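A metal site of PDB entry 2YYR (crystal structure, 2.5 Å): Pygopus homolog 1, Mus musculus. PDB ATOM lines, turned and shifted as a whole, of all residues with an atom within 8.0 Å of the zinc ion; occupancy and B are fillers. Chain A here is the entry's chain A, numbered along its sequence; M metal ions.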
ATOM      1  N   TYR A  10      17.920 -19.493  21.128  1.00  0.00           N
ATOM      2  CA  TYR A  10      16.655 -19.086  20.516  1.00  0.00           C
ATOM      3  C   TYR A  10      15.576 -20.091  20.922  1.00  0.00           C
ATOM      4  O   TYR A  10      15.143 -20.923  20.135  1.00  0.00           O
ATOM      5  CB  TYR A  10      16.788 -19.039  18.997  1.00  0.00           C
ATOM      6  CG  TYR A  10      17.704 -17.955  18.502  1.00  0.00           C
ATOM      7  CD1 TYR A  10      18.935 -18.258  17.911  1.00  0.00           C
ATOM      8  CD2 TYR A  10      17.338 -16.610  18.625  1.00  0.00           C
ATOM      9  CE1 TYR A  10      19.783 -17.242  17.449  1.00  0.00           C
ATOM     10  CE2 TYR A  10      18.186 -15.589  18.177  1.00  0.00           C
ATOM     11  CZ  TYR A  10      19.400 -15.917  17.592  1.00  0.00           C
ATOM     12  OH  TYR A  10      20.230 -14.920  17.151  1.00  0.00           O
ATOM     13  N   PRO A  11      15.129 -20.010  22.185  1.00  0.00           N
ATOM     14  CA  PRO A  11      14.101 -20.902  22.722  1.00  0.00           C
ATOM     15  C   PRO A  11      12.739 -20.662  22.075  1.00  0.00           C
ATOM     16  O   PRO A  11      12.299 -19.511  21.951  1.00  0.00           O
ATOM     17  CB  PRO A  11      14.044 -20.508  24.205  1.00  0.00           C
ATOM     18  CG  PRO A  11      15.354 -19.824  24.460  1.00  0.00           C
ATOM     19  CD  PRO A  11      15.555 -19.043  23.214  1.00  0.00           C
ATOM     20  N   CYS A  12      12.085 -21.727  21.647  1.00  0.00           N
ATOM     21  CA  CYS A  12      10.765 -21.620  21.037  1.00  0.00           C
ATOM     22  C   CYS A  12       9.812 -21.172  22.131  1.00  0.00           C
ATOM     23  O   CYS A  12       9.839 -21.716  23.231  1.00  0.00           O
ATOM     24  CB  CYS A  12      10.328 -22.978  20.478  1.00  0.00           C
ATOM     25  SG  CYS A  12       8.612 -23.045  19.902  1.00  0.00           S
ATOM     26  N   GLY A  13       8.997 -20.165  21.842  1.00  0.00           N
ATOM     27  CA  GLY A  13       8.060 -19.645  22.828  1.00  0.00           C
ATOM     28  C   GLY A  13       7.010 -20.621  23.322  1.00  0.00           C
ATOM     29  O   GLY A  13       6.276 -20.309  24.270  1.00  0.00           O
ATOM     30  N   ILE A  14       6.922 -21.792  22.703  1.00  0.00           N
ATOM     31  CA  ILE A  14       5.947 -22.796  23.109  1.00  0.00           C
ATOM     32  C   ILE A  14       6.597 -24.040  23.714  1.00  0.00           C
ATOM     33  O   ILE A  14       6.362 -24.363  24.884  1.00  0.00           O
ATOM     34  CB  ILE A  14       5.023 -23.187  21.919  1.00  0.00           C
ATOM     35  CG1 ILE A  14       4.149 -21.997  21.542  1.00  0.00           C
ATOM     36  CG2 ILE A  14       4.165 -24.403  22.275  1.00  0.00           C
ATOM     37  CD1 ILE A  14       3.344 -22.178  20.279  1.00  0.00           C
ATOM     38  N   CYS A  15       7.451 -24.717  22.942  1.00  0.00           N
ATOM     39  CA  CYS A  15       8.112 -25.928  23.420  1.00  0.00           C
ATOM     40  C   CYS A  15       9.423 -25.684  24.174  1.00  0.00           C
ATOM     41  O   CYS A  15       9.983 -26.620  24.744  1.00  0.00           O
ATOM     42  CB  CYS A  15       8.378 -26.875  22.253  1.00  0.00           C
ATOM     43  SG  CYS A  15       9.830 -26.404  21.298  1.00  0.00           S
ATOM     44  N   THR A  16       9.917 -24.445  24.142  1.00  0.00           N
ATOM     45  CA  THR A  16      11.162 -24.031  24.796  1.00  0.00           C
ATOM     46  C   THR A  16      12.420 -24.637  24.187  1.00  0.00           C
ATOM     47  O   THR A  16      13.532 -24.348  24.642  1.00  0.00           O
ATOM     48  CB  THR A  16      11.176 -24.316  26.337  1.00  0.00           C
ATOM     49  OG1 THR A  16      11.463 -25.699  26.593  1.00  0.00           O
ATOM     50  CG2 THR A  16       9.835 -23.941  26.990  1.00  0.00           C
ATOM     51  N   ASN A  17      12.258 -25.474  23.173  1.00  0.00           N
ATOM     52  CA  ASN A  17      13.399 -26.101  22.504  1.00  0.00           C
ATOM     53  C   ASN A  17      14.055 -25.133  21.513  1.00  0.00           C
ATOM     54  O   ASN A  17      13.460 -24.124  21.113  1.00  0.00           O
ATOM     55  CB  ASN A  17      12.972 -27.393  21.801  1.00  0.00           C
ATOM     56  CG  ASN A  17      12.409 -28.424  22.759  1.00  0.00           C
ATOM     57  OD1 ASN A  17      12.987 -28.682  23.814  1.00  0.00           O
ATOM     58  ND2 ASN A  17      11.282 -29.020  22.390  1.00  0.00           N
ATOM     59  N   GLU A  18      15.276 -25.451  21.117  1.00  0.00           N
ATOM     60  CA  GLU A  18      16.061 -24.644  20.193  1.00  0.00           C
ATOM     61  C   GLU A  18      15.430 -24.466  18.814  1.00  0.00           C
ATOM     62  O   GLU A  18      14.942 -25.429  18.225  1.00  0.00           O
ATOM     63  CB  GLU A  18      17.452 -25.260  20.027  1.00  0.00           C
ATOM     64  CG  GLU A  18      18.609 -24.314  20.283  1.00  0.00           C
ATOM     65  CD  GLU A  18      18.698 -23.185  19.269  1.00  0.00           C
ATOM     66  OE1 GLU A  18      18.306 -22.050  19.612  1.00  0.00           O
ATOM     67  OE2 GLU A  18      19.176 -23.440  18.143  1.00  0.00           O
ATOM     68  N   VAL A  19      15.444 -23.238  18.323  1.00  0.00           N
ATOM     69  CA  VAL A  19      14.923 -22.946  16.993  1.00  0.00           C
ATOM     70  C   VAL A  19      16.137 -22.828  16.064  1.00  0.00           C
ATOM     71  O   VAL A  19      16.865 -21.838  16.102  1.00  0.00           O
ATOM     72  CB  VAL A  19      14.100 -21.633  16.964  1.00  0.00           C
ATOM     73  CG1 VAL A  19      13.705 -21.290  15.554  1.00  0.00           C
ATOM     74  CG2 VAL A  19      12.846 -21.796  17.810  1.00  0.00           C
ATOM     75  N   GLN A  23      14.872 -25.193  10.426  1.00  0.00           N
ATOM     76  CA  GLN A  23      13.514 -25.468  10.879  1.00  0.00           C
ATOM     77  C   GLN A  23      12.582 -24.328  10.494  1.00  0.00           C
ATOM     78  O   GLN A  23      13.009 -23.177  10.377  1.00  0.00           O
ATOM     79  CB  GLN A  23      13.458 -25.659  12.393  1.00  0.00           C
ATOM     80  CG  GLN A  23      14.275 -26.812  12.936  1.00  0.00           C
ATOM     81  CD  GLN A  23      14.206 -26.907  14.446  1.00  0.00           C
ATOM     82  OE1 GLN A  23      14.353 -25.909  15.143  1.00  0.00           O
ATOM     83  NE2 GLN A  23      13.984 -28.106  14.958  1.00  0.00           N
ATOM     84  N   ASP A  24      11.309 -24.659  10.286  1.00  0.00           N
ATOM     85  CA  ASP A  24      10.293 -23.658   9.954  1.00  0.00           C
ATOM     86  C   ASP A  24       9.949 -22.958  11.257  1.00  0.00           C
ATOM     87  O   ASP A  24       9.486 -23.584  12.203  1.00  0.00           O
ATOM     88  CB  ASP A  24       9.022 -24.312   9.411  1.00  0.00           C
ATOM     89  CG  ASP A  24       9.214 -24.913   8.030  1.00  0.00           C
ATOM     90  OD1 ASP A  24      10.260 -24.667   7.395  1.00  0.00           O
ATOM     91  OD2 ASP A  24       8.290 -25.625   7.584  1.00  0.00           O
ATOM     92  N   ALA A  25      10.201 -21.657  11.318  1.00  0.00           N
ATOM     93  CA  ALA A  25       9.891 -20.895  12.522  1.00  0.00           C
ATOM     94  C   ALA A  25       9.499 -19.486  12.135  1.00  0.00           C
ATOM     95  O   ALA A  25       9.877 -18.993  11.079  1.00  0.00           O
ATOM     96  CB  ALA A  25      11.072 -20.874  13.456  1.00  0.00           C
ATOM     97  N   TRP A  35      10.974 -16.451  18.899  1.00  0.00           N
ATOM     98  CA  TRP A  35      10.766 -17.352  17.764  1.00  0.00           C
ATOM     99  C   TRP A  35       9.844 -18.485  18.162  1.00  0.00           C
ATOM    100  O   TRP A  35       9.911 -18.986  19.294  1.00  0.00           O
ATOM    101  CB  TRP A  35      12.093 -17.903  17.256  1.00  0.00           C
ATOM    102  CG  TRP A  35      12.917 -16.921  16.474  1.00  0.00           C
ATOM    103  CD1 TRP A  35      13.909 -16.122  16.955  1.00  0.00           C
ATOM    104  CD2 TRP A  35      12.822 -16.642  15.067  1.00  0.00           C
ATOM    105  NE1 TRP A  35      14.457 -15.374  15.937  1.00  0.00           N
ATOM    106  CE2 TRP A  35      13.804 -15.674  14.773  1.00  0.00           C
ATOM    107  CE3 TRP A  35      12.010 -17.131  14.037  1.00  0.00           C
ATOM    108  CZ2 TRP A  35      13.996 -15.165  13.478  1.00  0.00           C
ATOM    109  CZ3 TRP A  35      12.202 -16.632  12.751  1.00  0.00           C
ATOM    110  CH2 TRP A  35      13.184 -15.656  12.485  1.00  0.00           C
ATOM    111  N   PHE A  36       8.968 -18.895  17.249  1.00  0.00           N
ATOM    112  CA  PHE A  36       8.028 -19.978  17.509  1.00  0.00           C
ATOM    113  C   PHE A  36       8.052 -20.965  16.346  1.00  0.00           C
ATOM    114  O   PHE A  36       7.864 -20.571  15.201  1.00  0.00           O
ATOM    115  CB  PHE A  36       6.596 -19.433  17.636  1.00  0.00           C
ATOM    116  CG  PHE A  36       6.400 -18.519  18.819  1.00  0.00           C
ATOM    117  CD1 PHE A  36       6.900 -17.227  18.810  1.00  0.00           C
ATOM    118  CD2 PHE A  36       5.693 -18.963  19.928  1.00  0.00           C
ATOM    119  CE1 PHE A  36       6.710 -16.383  19.895  1.00  0.00           C
ATOM    120  CE2 PHE A  36       5.491 -18.131  21.032  1.00  0.00           C
ATOM    121  CZ  PHE A  36       6.003 -16.826  21.004  1.00  0.00           C
ATOM    122  N   HIS A  37       8.280 -22.240  16.659  1.00  0.00           N
ATOM    123  CA  HIS A  37       8.293 -23.273  15.619  1.00  0.00           C
ATOM    124  C   HIS A  37       6.934 -23.262  14.927  1.00  0.00           C
ATOM    125  O   HIS A  37       5.901 -23.120  15.585  1.00  0.00           O
ATOM    126  CB  HIS A  37       8.535 -24.652  16.226  1.00  0.00           C
ATOM    127  CG  HIS A  37       9.960 -24.903  16.633  1.00  0.00           C
ATOM    128  ND1 HIS A  37      10.320 -25.198  17.942  1.00  0.00           N
ATOM    129  CD2 HIS A  37      11.112 -24.934  15.914  1.00  0.00           C
ATOM    130  CE1 HIS A  37      11.627 -25.402  17.991  1.00  0.00           C
ATOM    131  NE2 HIS A  37      12.123 -25.250  16.788  1.00  0.00           N
ATOM    132  N   ARG A  38       6.936 -23.397  13.599  1.00  0.00           N
ATOM    133  CA  ARG A  38       5.687 -23.420  12.842  1.00  0.00           C
ATOM    134  C   ARG A  38       4.753 -24.507  13.374  1.00  0.00           C
ATOM    135  O   ARG A  38       3.580 -24.255  13.657  1.00  0.00           O
ATOM    136  CB  ARG A  38       5.956 -23.650  11.357  1.00  0.00           C
ATOM    137  CG  ARG A  38       4.713 -23.814  10.522  1.00  0.00           C
ATOM    138  CD  ARG A  38       5.036 -24.252   9.110  1.00  0.00           C
ATOM    139  NE  ARG A  38       5.743 -25.527   9.070  1.00  0.00           N
ATOM    140  CZ  ARG A  38       5.161 -26.713   9.204  1.00  0.00           C
ATOM    141  NH1 ARG A  38       3.852 -26.809   9.386  1.00  0.00           N
ATOM    142  NH2 ARG A  38       5.889 -27.825   9.126  1.00  0.00           N
ATOM    143  N   ILE A  39       5.304 -25.709  13.557  1.00  0.00           N
ATOM    144  CA  ILE A  39       4.556 -26.850  14.053  1.00  0.00           C
ATOM    145  C   ILE A  39       3.998 -26.587  15.455  1.00  0.00           C
ATOM    146  O   ILE A  39       2.848 -26.929  15.750  1.00  0.00           O
ATOM    147  CB  ILE A  39       5.424 -28.139  14.017  1.00  0.00           C
ATOM    148  CG1 ILE A  39       5.677 -28.542  12.551  1.00  0.00           C
ATOM    149  CG2 ILE A  39       4.746 -29.282  14.778  1.00  0.00           C
ATOM    150  CD1 ILE A  39       6.768 -29.602  12.370  1.00  0.00           C
ATOM    151  N   CYS A  40       4.796 -25.950  16.305  1.00  0.00           N
ATOM    152  CA  CYS A  40       4.365 -25.651  17.661  1.00  0.00           C
ATOM    153  C   CYS A  40       3.143 -24.721  17.716  1.00  0.00           C
ATOM    154  O   CYS A  40       2.258 -24.921  18.522  1.00  0.00           O
ATOM    155  CB  CYS A  40       5.516 -25.061  18.479  1.00  0.00           C
ATOM    156  SG  CYS A  40       6.812 -26.276  18.855  1.00  0.00           S
ATOM    157  N   THR A  41       3.111 -23.722  16.834  1.00  0.00           N
ATOM    158  CA  THR A  41       1.987 -22.779  16.784  1.00  0.00           C
ATOM    159  C   THR A  41       0.755 -23.365  16.089  1.00  0.00           C
ATOM    160  O   THR A  41      -0.331 -22.785  16.148  1.00  0.00           O
ATOM    161  CB  THR A  41       2.380 -21.472  16.058  1.00  0.00           C
ATOM    162  OG1 THR A  41       2.754 -21.742  14.701  1.00  0.00           O
ATOM    163  CG2 THR A  41       3.536 -20.806  16.752  1.00  0.00           C
HETATM  164 ZN    ZN M   1       8.773 -25.326  19.381  1.00  0.00          ZN
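The side-chain sulfur of Cys 12 sits close to the backbone NH of Ile 14 (3.5 Å).
NE2 of His 37 is in hydrogen-bond range of OE1 of Gln 23.
The backbone NH (N) of Cys 12 lies within hydrogen-bond range of the backbone carbonyl oxygen (O) of Asn 17 (2.8 Å).
NE2 of His 37 is in hydrogen-bond range of O of Glu 18, at 3.2 Å.
ND2 of Asn 17 lies close to SG of Cys 15 (3.2 Å).
ND1 of His 37 binds the zinc ion, at 2.1 Å.
SG of Cys 40 binds the zinc ion, 2.2 Å away.
The zinc ion is bound by SG of Cys 12 (2.3 Å).
The zinc ion is bound by SG of Cys 15 (2.4 Å).
Four residues have an atom within 4 Å of the zinc ion: Cys 12, Cys 15, His 37 and Cys 40.
The nearest printed residue that does not touch the zinc ion is Thr 16 (5.0 Å).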
